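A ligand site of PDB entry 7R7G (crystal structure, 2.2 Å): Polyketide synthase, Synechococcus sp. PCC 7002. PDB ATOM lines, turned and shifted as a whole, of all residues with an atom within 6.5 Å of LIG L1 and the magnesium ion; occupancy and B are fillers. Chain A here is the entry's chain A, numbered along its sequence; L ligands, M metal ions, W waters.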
ATOM      1  N   TYR A 170     -30.779 -19.531 -18.292  1.00  0.00           N
ATOM      2  CA  TYR A 170     -30.300 -19.596 -16.907  1.00  0.00           C
ATOM      3  C   TYR A 170     -29.060 -20.481 -16.826  1.00  0.00           C
ATOM      4  O   TYR A 170     -29.036 -21.515 -17.495  1.00  0.00           O
ATOM      5  CB  TYR A 170     -31.409 -19.978 -15.919  1.00  0.00           C
ATOM      6  CG  TYR A 170     -32.230 -18.824 -15.394  1.00  0.00           C
ATOM      7  CD1 TYR A 170     -33.150 -18.192 -16.206  1.00  0.00           C
ATOM      8  CD2 TYR A 170     -32.096 -18.393 -14.088  1.00  0.00           C
ATOM      9  CE1 TYR A 170     -33.915 -17.133 -15.733  1.00  0.00           C
ATOM     10  CE2 TYR A 170     -32.860 -17.340 -13.598  1.00  0.00           C
ATOM     11  CZ  TYR A 170     -33.766 -16.711 -14.424  1.00  0.00           C
ATOM     12  OH  TYR A 170     -34.517 -15.670 -13.975  1.00  0.00           O
ATOM     13  N   THR A 171     -28.095 -20.065 -16.011  1.00  0.00           N
ATOM     14  CA  THR A 171     -26.840 -20.815 -15.819  1.00  0.00           C
ATOM     15  C   THR A 171     -27.156 -22.094 -15.061  1.00  0.00           C
ATOM     16  O   THR A 171     -28.162 -22.131 -14.375  1.00  0.00           O
ATOM     17  CB  THR A 171     -25.785 -19.912 -15.167  1.00  0.00           C
ATOM     18  OG1 THR A 171     -26.162 -19.617 -13.828  1.00  0.00           O
ATOM     19  CG2 THR A 171     -25.577 -18.626 -15.932  1.00  0.00           C
ATOM     20  N   SER A 172     -26.272 -23.089 -15.141  1.00  0.00           N
ATOM     21  CA  SER A 172     -26.491 -24.404 -14.493  1.00  0.00           C
ATOM     22  C   SER A 172     -26.532 -24.290 -12.960  1.00  0.00           C
ATOM     23  O   SER A 172     -27.216 -25.111 -12.349  1.00  0.00           O
ATOM     24  CB  SER A 172     -25.456 -25.368 -14.940  1.00  0.00           C
ATOM     25  OG  SER A 172     -24.206 -25.081 -14.328  1.00  0.00           O
ATOM     26  N   GLY A 173     -25.829 -23.325 -12.379  1.00  0.00           N
ATOM     27  CA  GLY A 173     -25.783 -23.204 -10.918  1.00  0.00           C
ATOM     28  C   GLY A 173     -24.653 -24.005 -10.301  1.00  0.00           C
ATOM     29  O   GLY A 173     -24.758 -24.323  -9.110  1.00  0.00           O
ATOM     30  N   SER A 174     -23.620 -24.291 -11.071  1.00  0.00           N
ATOM     31  CA  SER A 174     -22.489 -25.098 -10.564  1.00  0.00           C
ATOM     32  C   SER A 174     -21.686 -24.281  -9.546  1.00  0.00           C
ATOM     33  O   SER A 174     -21.209 -24.871  -8.578  1.00  0.00           O
ATOM     34  CB  SER A 174     -21.662 -25.576 -11.727  1.00  0.00           C
ATOM     35  OG  SER A 174     -21.383 -24.519 -12.624  1.00  0.00           O
ATOM     36  N   THR A 175     -21.573 -22.964  -9.750  1.00  0.00           N
ATOM     37  CA  THR A 175     -20.698 -22.119  -8.893  1.00  0.00           C
ATOM     38  C   THR A 175     -21.525 -21.262  -7.929  1.00  0.00           C
ATOM     39  O   THR A 175     -20.928 -20.670  -7.029  1.00  0.00           O
ATOM     40  CB  THR A 175     -19.763 -21.256  -9.750  1.00  0.00           C
ATOM     41  OG1 THR A 175     -20.505 -20.176 -10.310  1.00  0.00           O
ATOM     42  CG2 THR A 175     -19.035 -22.045 -10.824  1.00  0.00           C
ATOM     43  N   GLY A 176     -22.831 -21.220  -8.121  1.00  0.00           N
ATOM     44  CA  GLY A 176     -23.719 -20.447  -7.224  1.00  0.00           C
ATOM     45  C   GLY A 176     -25.173 -20.662  -7.585  1.00  0.00           C
ATOM     46  O   GLY A 176     -25.534 -21.807  -7.883  1.00  0.00           O
ATOM     47  N   ASP A 177     -25.971 -19.609  -7.521  1.00  0.00           N
ATOM     48  CA  ASP A 177     -27.399 -19.733  -7.876  1.00  0.00           C
ATOM     49  C   ASP A 177     -27.516 -19.527  -9.381  1.00  0.00           C
ATOM     50  O   ASP A 177     -26.723 -18.754  -9.919  1.00  0.00           O
ATOM     51  CB  ASP A 177     -28.285 -18.764  -7.092  1.00  0.00           C
ATOM     52  CG  ASP A 177     -28.417 -19.129  -5.622  1.00  0.00           C
ATOM     53  OD1 ASP A 177     -28.074 -20.277  -5.274  1.00  0.00           O
ATOM     54  OD2 ASP A 177     -28.860 -18.261  -4.854  1.00  0.00           O
ATOM     55  N   PRO A 178     -28.439 -20.223 -10.093  1.00  0.00           N
ATOM     56  CA  PRO A 178     -28.637 -19.929 -11.498  1.00  0.00           C
ATOM     57  C   PRO A 178     -28.898 -18.437 -11.707  1.00  0.00           C
ATOM     58  O   PRO A 178     -29.699 -17.882 -11.013  1.00  0.00           O
ATOM     59  CB  PRO A 178     -29.832 -20.831 -11.877  1.00  0.00           C
ATOM     60  CG  PRO A 178     -29.663 -22.026 -10.983  1.00  0.00           C
ATOM     61  CD  PRO A 178     -29.244 -21.390  -9.674  1.00  0.00           C
ATOM     62  N   LYS A 179     -28.208 -17.841 -12.667  1.00  0.00           N
ATOM     63  CA  LYS A 179     -28.427 -16.418 -13.001  1.00  0.00           C
ATOM     64  C   LYS A 179     -29.100 -16.342 -14.377  1.00  0.00           C
ATOM     65  O   LYS A 179     -28.872 -17.231 -15.192  1.00  0.00           O
ATOM     66  CB  LYS A 179     -27.106 -15.653 -12.976  1.00  0.00           C
ATOM     67  CG  LYS A 179     -26.149 -16.039 -11.861  1.00  0.00           C
ATOM     68  CD  LYS A 179     -24.728 -15.612 -12.141  1.00  0.00           C
ATOM     69  CE  LYS A 179     -24.092 -16.422 -13.243  1.00  0.00           C
ATOM     70  NZ  LYS A 179     -23.069 -17.350 -12.713  1.00  0.00           N
ATOM     71  N   ASP A 216     -27.795 -24.143 -23.510  1.00  0.00           N
ATOM     72  CA  ASP A 216     -26.498 -24.191 -24.235  1.00  0.00           C
ATOM     73  C   ASP A 216     -26.472 -25.002 -25.528  1.00  0.00           C
ATOM     74  O   ASP A 216     -27.318 -24.726 -26.413  1.00  0.00           O
ATOM     75  CB  ASP A 216     -25.323 -24.513 -23.291  1.00  0.00           C
ATOM     76  CG  ASP A 216     -25.523 -25.721 -22.397  1.00  0.00           C
ATOM     77  OD1 ASP A 216     -25.466 -26.849 -22.915  1.00  0.00           O
ATOM     78  OD2 ASP A 216     -25.750 -25.517 -21.188  1.00  0.00           O
ATOM     79  N   MET A 325     -19.980 -19.945 -23.180  1.00  0.00           N
ATOM     80  CA  MET A 325     -20.888 -19.945 -22.016  1.00  0.00           C
ATOM     81  C   MET A 325     -22.217 -19.289 -22.397  1.00  0.00           C
ATOM     82  O   MET A 325     -22.329 -18.815 -23.522  1.00  0.00           O
ATOM     83  CB  MET A 325     -20.275 -19.138 -20.868  1.00  0.00           C
ATOM     84  CG  MET A 325     -19.912 -17.738 -21.258  1.00  0.00           C
ATOM     85  SD  MET A 325     -18.397 -17.212 -20.474  1.00  0.00           S
ATOM     86  CE  MET A 325     -18.895 -17.337 -18.763  1.00  0.00           C
ATOM     87  N   ALA A 326     -23.148 -19.194 -21.444  1.00  0.00           N
ATOM     88  CA  ALA A 326     -24.459 -18.555 -21.692  1.00  0.00           C
ATOM     89  C   ALA A 326     -24.317 -17.047 -21.813  1.00  0.00           C
ATOM     90  O   ALA A 326     -25.074 -16.461 -22.599  1.00  0.00           O
ATOM     91  CB  ALA A 326     -25.389 -18.939 -20.589  1.00  0.00           C
ATOM     92  N   GLU A 327     -23.368 -16.449 -21.083  1.00  0.00           N
ATOM     93  CA  GLU A 327     -23.140 -14.978 -21.126  1.00  0.00           C
ATOM     94  C   GLU A 327     -22.582 -14.603 -22.499  1.00  0.00           C
ATOM     95  O   GLU A 327     -22.623 -13.409 -22.850  1.00  0.00           O
ATOM     96  CB  GLU A 327     -22.197 -14.563 -19.995  1.00  0.00           C
ATOM     97  CG  GLU A 327     -22.789 -14.724 -18.605  1.00  0.00           C
ATOM     98  CD  GLU A 327     -22.740 -16.119 -18.005  1.00  0.00           C
ATOM     99  OE1 GLU A 327     -22.201 -17.031 -18.657  1.00  0.00           O
ATOM    100  OE2 GLU A 327     -23.235 -16.295 -16.882  1.00  0.00           O
ATOM    101  N   TYR A 411     -27.304  -9.693 -16.599  1.00  0.00           N
ATOM    102  CA  TYR A 411     -28.059 -10.661 -15.771  1.00  0.00           C
ATOM    103  C   TYR A 411     -29.413 -10.052 -15.409  1.00  0.00           C
ATOM    104  O   TYR A 411     -29.460  -8.892 -15.015  1.00  0.00           O
ATOM    105  CB  TYR A 411     -27.286 -11.128 -14.548  1.00  0.00           C
ATOM    106  CG  TYR A 411     -25.991 -11.850 -14.786  1.00  0.00           C
ATOM    107  CD1 TYR A 411     -25.950 -13.053 -15.457  1.00  0.00           C
ATOM    108  CD2 TYR A 411     -24.793 -11.338 -14.303  1.00  0.00           C
ATOM    109  CE1 TYR A 411     -24.757 -13.724 -15.666  1.00  0.00           C
ATOM    110  CE2 TYR A 411     -23.601 -11.995 -14.501  1.00  0.00           C
ATOM    111  CZ  TYR A 411     -23.583 -13.193 -15.181  1.00  0.00           C
ATOM    112  OH  TYR A 411     -22.392 -13.836 -15.369  1.00  0.00           O
ATOM    113  N   THR A 435     -15.551 -13.830 -17.716  1.00  0.00           N
ATOM    114  CA  THR A 435     -16.165 -15.177 -17.831  1.00  0.00           C
ATOM    115  C   THR A 435     -16.077 -15.910 -16.488  1.00  0.00           C
ATOM    116  O   THR A 435     -16.876 -16.837 -16.272  1.00  0.00           O
ATOM    117  CB  THR A 435     -15.444 -15.974 -18.925  1.00  0.00           C
ATOM    118  OG1 THR A 435     -14.099 -16.193 -18.486  1.00  0.00           O
ATOM    119  CG2 THR A 435     -15.430 -15.255 -20.251  1.00  0.00           C
ATOM    120  N   ASP A 437     -13.655 -17.628 -15.901  1.00  0.00           N
ATOM    121  CA  ASP A 437     -12.872 -18.823 -16.312  1.00  0.00           C
ATOM    122  C   ASP A 437     -11.402 -18.428 -16.425  1.00  0.00           C
ATOM    123  O   ASP A 437     -11.124 -17.372 -17.015  1.00  0.00           O
ATOM    124  CB  ASP A 437     -13.357 -19.389 -17.644  1.00  0.00           C
ATOM    125  CG  ASP A 437     -14.775 -19.911 -17.578  1.00  0.00           C
ATOM    126  OD1 ASP A 437     -15.008 -20.874 -16.827  1.00  0.00           O
ATOM    127  OD2 ASP A 437     -15.637 -19.350 -18.277  1.00  0.00           O
ATOM    128  N   ARG A 451     -12.299 -22.802 -13.437  1.00  0.00           N
ATOM    129  CA  ARG A 451     -13.173 -21.719 -12.946  1.00  0.00           C
ATOM    130  C   ARG A 451     -12.529 -21.038 -11.741  1.00  0.00           C
ATOM    131  O   ARG A 451     -12.046 -21.754 -10.865  1.00  0.00           O
ATOM    132  CB  ARG A 451     -14.538 -22.291 -12.580  1.00  0.00           C
ATOM    133  CG  ARG A 451     -15.177 -23.151 -13.656  1.00  0.00           C
ATOM    134  CD  ARG A 451     -16.683 -23.079 -13.501  1.00  0.00           C
ATOM    135  NE  ARG A 451     -17.384 -24.272 -13.944  1.00  0.00           N
ATOM    136  CZ  ARG A 451     -18.507 -24.244 -14.646  1.00  0.00           C
ATOM    137  NH1 ARG A 451     -19.042 -23.080 -14.972  1.00  0.00           N
ATOM    138  NH2 ARG A 451     -19.088 -25.363 -15.005  1.00  0.00           N
ATOM    139  N   LYS A 453     -13.954 -19.171  -9.320  1.00  0.00           N
ATOM    140  CA  LYS A 453     -14.732 -19.350  -8.074  1.00  0.00           C
ATOM    141  C   LYS A 453     -14.512 -20.762  -7.489  1.00  0.00           C
ATOM    142  O   LYS A 453     -14.677 -20.902  -6.283  1.00  0.00           O
ATOM    143  CB  LYS A 453     -16.188 -18.986  -8.329  1.00  0.00           C
ATOM    144  CG  LYS A 453     -16.461 -17.529  -8.666  1.00  0.00           C
ATOM    145  CD  LYS A 453     -17.928 -17.267  -8.937  1.00  0.00           C
ATOM    146  CE  LYS A 453     -18.837 -18.066  -8.028  1.00  0.00           C
ATOM    147  NZ  LYS A 453     -19.705 -17.193  -7.218  1.00  0.00           N
ATOM    148  N   THR A 546     -26.187 -30.313 -10.569  1.00  0.00           N
ATOM    149  CA  THR A 546     -27.160 -29.425 -11.266  1.00  0.00           C
ATOM    150  C   THR A 546     -28.187 -30.308 -11.992  1.00  0.00           C
ATOM    151  O   THR A 546     -28.054 -31.534 -11.925  1.00  0.00           O
ATOM    152  CB  THR A 546     -26.446 -28.522 -12.272  1.00  0.00           C
ATOM    153  OG1 THR A 546     -25.904 -29.342 -13.307  1.00  0.00           O
ATOM    154  CG2 THR A 546     -25.350 -27.678 -11.653  1.00  0.00           C
ATOM    155  N   LYS A 550     -23.836 -31.410 -13.681  1.00  0.00           N
ATOM    156  CA  LYS A 550     -22.585 -30.750 -13.250  1.00  0.00           C
ATOM    157  C   LYS A 550     -22.542 -30.691 -11.723  1.00  0.00           C
ATOM    158  O   LYS A 550     -23.508 -30.251 -11.120  1.00  0.00           O
ATOM    159  CB  LYS A 550     -22.470 -29.336 -13.824  1.00  0.00           C
ATOM    160  CG  LYS A 550     -21.925 -29.211 -15.238  1.00  0.00           C
ATOM    161  CD  LYS A 550     -22.163 -27.828 -15.806  1.00  0.00           C
ATOM    162  CE  LYS A 550     -21.432 -27.579 -17.111  1.00  0.00           C
ATOM    163  NZ  LYS A 550     -21.937 -26.374 -17.796  1.00  0.00           N
HETATM  164  P1  LIG L   1     -22.871 -21.091 -13.209  1.00  0.00           P
HETATM  165  O1  LIG L   1     -24.294 -21.177 -12.769  1.00  0.00           O
HETATM  166  O2  LIG L   1     -21.931 -21.230 -12.081  1.00  0.00           O
HETATM  167  O3  LIG L   1     -22.595 -19.900 -14.055  1.00  0.00           O
HETATM  168  O4  LIG L   1     -22.581 -22.371 -14.100  1.00  0.00           O
HETATM  169  P2  LIG L   1     -22.275 -22.514 -15.654  1.00  0.00           P
HETATM  170  O5  LIG L   1     -23.560 -22.095 -16.276  1.00  0.00           O
HETATM  171  O6  LIG L   1     -21.933 -23.951 -15.872  1.00  0.00           O
HETATM  172  O7  LIG L   1     -21.141 -21.590 -15.969  1.00  0.00           O
HETATM  173  C1  LG2 L   2     -21.701 -23.586 -23.107  1.00  0.00           C
HETATM  174  C2  LG2 L   2     -20.178 -23.852 -25.081  1.00  0.00           C
HETATM  175  C3  LG2 L   2     -20.415 -25.195 -27.963  1.00  0.00           C
HETATM  176  C4  LG2 L   2     -20.649 -24.862 -29.425  1.00  0.00           C
HETATM  177  C5  LG2 L   2     -20.971 -26.098 -30.253  1.00  0.00           C
HETATM  178  C6  LG2 L   2     -22.857 -26.039 -31.931  1.00  0.00           C
HETATM  179  C7  LG2 L   2     -24.221 -26.916 -33.892  1.00  0.00           C
HETATM  180  C8  LG2 L   2     -24.673 -28.245 -36.002  1.00  0.00           C
HETATM  181  C9  LG2 L   2     -14.140 -25.871 -22.327  1.00  0.00           C
HETATM  182  C10 LG2 L   2     -15.350 -25.390 -21.799  1.00  0.00           C
HETATM  183  C11 LG2 L   2     -15.476 -25.312 -20.437  1.00  0.00           C
HETATM  184  C12 LG2 L   2     -17.232 -24.602 -18.856  1.00  0.00           C
HETATM  185  C13 LG2 L   2     -18.815 -22.951 -18.443  1.00  0.00           C
HETATM  186  C14 LG2 L   2     -20.075 -22.442 -19.090  1.00  0.00           C
HETATM  187  C15 LG2 L   2     -21.835 -23.927 -21.630  1.00  0.00           C
HETATM  188  C16 LG2 L   2     -20.673 -24.481 -23.786  1.00  0.00           C
HETATM  189  C17 LG2 L   2     -19.182 -24.695 -25.845  1.00  0.00           C
HETATM  190  C18 LG2 L   2     -19.295 -24.375 -27.329  1.00  0.00           C
HETATM  191  C19 LG2 L   2     -22.463 -26.285 -30.489  1.00  0.00           C
HETATM  192  C20 LG2 L   2     -23.728 -27.162 -32.483  1.00  0.00           C
HETATM  193  C21 LG2 L   2     -24.884 -28.147 -34.488  1.00  0.00           C
HETATM  194  C22 LG2 L   2     -25.981 -28.267 -36.786  1.00  0.00           C
HETATM  195  C23 LG2 L   2     -17.804 -22.318 -18.909  1.00  0.00           C
HETATM  196  C24 LG2 L   2     -16.682 -23.215 -18.446  1.00  0.00           C
HETATM  197  C25 LG2 L   2     -17.293 -24.615 -21.364  1.00  0.00           C
HETATM  198  C26 LG2 L   2     -13.349 -26.141 -20.192  1.00  0.00           C
HETATM  199  N1  LG2 L   2     -13.938 -25.961 -23.754  1.00  0.00           N
HETATM  200  N2  LG2 L   2     -16.698 -24.841 -20.211  1.00  0.00           N
HETATM  201  N3  LG2 L   2     -16.489 -24.948 -22.343  1.00  0.00           N
HETATM  202  N4  LG2 L   2     -14.463 -25.705 -19.673  1.00  0.00           N
HETATM  203  N5  LG2 L   2     -13.182 -26.227 -21.500  1.00  0.00           N
HETATM  204  O1  LG2 L   2     -18.505 -24.479 -18.853  1.00  0.00           O
HETATM  205  O2  LG2 L   2     -21.114 -23.299 -18.740  1.00  0.00           O
HETATM  206  O3  LG2 L   2     -23.626 -23.718 -18.483  1.00  0.00           O
HETATM  207  O4  LG2 L   2     -22.847 -23.347 -20.850  1.00  0.00           O
HETATM  208  O5  LG2 L   2     -21.066 -24.712 -21.180  1.00  0.00           O
HETATM  209  O6  LG2 L   2     -22.863 -21.457 -19.077  1.00  0.00           O
HETATM  210  O7  LG2 L   2     -17.730 -20.954 -18.305  1.00  0.00           O
HETATM  211  O8  LG2 L   2     -16.544 -23.151 -17.095  1.00  0.00           O
HETATM  212  P1  LG2 L   2     -22.623 -22.930 -19.272  1.00  0.00           P
HETATM  213 MG    MG M   1     -20.697 -19.646 -14.918  1.00  0.00          MG
HETATM  214  O   HOH W   1     -19.307 -19.736 -16.485  1.00  0.00           O
HETATM  215  O   HOH W   2     -24.338 -19.120 -10.934  1.00  0.00           O
HETATM  216  O   HOH W   3     -21.246 -17.699 -15.252  1.00  0.00           O
HETATM  217  O   HOH W   4     -21.849 -19.336 -17.183  1.00  0.00           O
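The backbone NH of Lys 179 sits at hydrogen-bond distance from the side-chain hydroxyl of Thr 171, at 2.9 Å. The guanidinium group (NH2) of Arg 451 sits at hydrogen-bond distance from the side-chain hydroxyl (OG) of Ser 174 (3.4 Å). OG of Ser 174 lies within hydrogen-bond range of OG of Ser 172, 3.3 Å away. The side-chain hydroxyl (OG1) of Thr 546 sits at hydrogen-bond distance from the backbone NH (N) of Lys 550.
Eight residues have an atom within 4 Å of LIG L1: Thr 171, Ser 172, Gly 173, Ser 174, Thr 175, Lys 179, Arg 451 and Lys 550. The nearest printed residue that does not touch LIG L1 is Gly 176 (4.1 Å).
Residues that only touch the magnesium ion: Arg 451 (3.8 Å) and Lys 179 (3.97 Å). Of the 21 residues printed, 2 come within 4 Å of the magnesium ion.
Water W4 lies within hydrogen-bond range of the side-chain carboxylate (OE1) of Glu 327 (2.8 Å), an oxygen (O6) of LG2 L2 (3.0 Å) and an oxygen (O5) of LIG L1 (3.4 Å). Water W3 lies within hydrogen-bond range of OE2 of Glu 327 (2.9 Å) and NZ of Lys 179 (3.1 Å). Water W2 lies within hydrogen-bond range of O of Asp 177 (2.6 Å), O1 of LIG L1 (2.8 Å), NZ of Lys 179 (2.8 Å) and OG1 of Thr 171 (3.5 Å).
An oxygen (O5) of LIG L1 sits close to an oxygen (O3) of LG2 L2 (2.7 Å).
Water W3 binds the magnesium ion (2.1 Å). Water W1 is bound to the magnesium ion, 2.1 Å away. O3 of LIG L1 binds the magnesium ion (2.1 Å). The magnesium ion is bound by an oxygen (O7) of LIG L1, at 2.3 Å. The magnesium ion is bound by water W4, at 2.6 Å. The magnesium ion has five donor atoms within binding distance.
The backbone NH (N) of Thr 175 sits at hydrogen-bond distance from an oxygen (O2) of LIG L1 (2.9 Å). The side-chain hydroxyl of Thr 175 lies within hydrogen-bond range of an oxygen (O2) of LIG L1, 2.5 Å away. The side-chain hydroxyl (OG1) of Thr 171 is in hydrogen-bond range of an oxygen (O1) of LIG L1, at 2.7 Å. The backbone NH (N) of Gly 173 is in hydrogen-bond range of an oxygen (O1) of LIG L1, at 2.7 Å. O6 of LIG L1 lies within salt-bridge range of NH1 of Arg 451. The side-chain hydroxyl (OG) of Ser 174 sits at hydrogen-bond distance from an oxygen (O4) of LIG L1, at 2.9 Å. An oxygen (O3) of LIG L1 lies close to the side-chain amino group (NZ) of Lys 179 (2.9 Å). N of Ser 172 lies within hydrogen-bond range of O5 of LIG L1, 3.1 Å away. The side-chain hydroxyl (OG) of Ser 172 is in hydrogen-bond range of an oxygen (O6) of LIG L1, 3.0 Å away. NZ of Lys 550 lies within salt-bridge range of O6 of LIG L1. An oxygen (O8) of LG2 L2 is in hydrogen-bond range of the guanidinium group (NH1) of Arg 451, 3.3 Å away. The side-chain amino group (NZ) of Lys 550 is in salt-bridge range of an oxygen (O3) of LG2 L2. An oxygen (O6) of LG2 L2 sits at hydrogen-bond distance from the backbone NH (N) of Ala 326, 3.3 Å away. The side-chain carboxylate (OD2) of Asp 437 sits at hydrogen-bond distance from an oxygen (O7) of LG2 L2 (2.6 Å).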
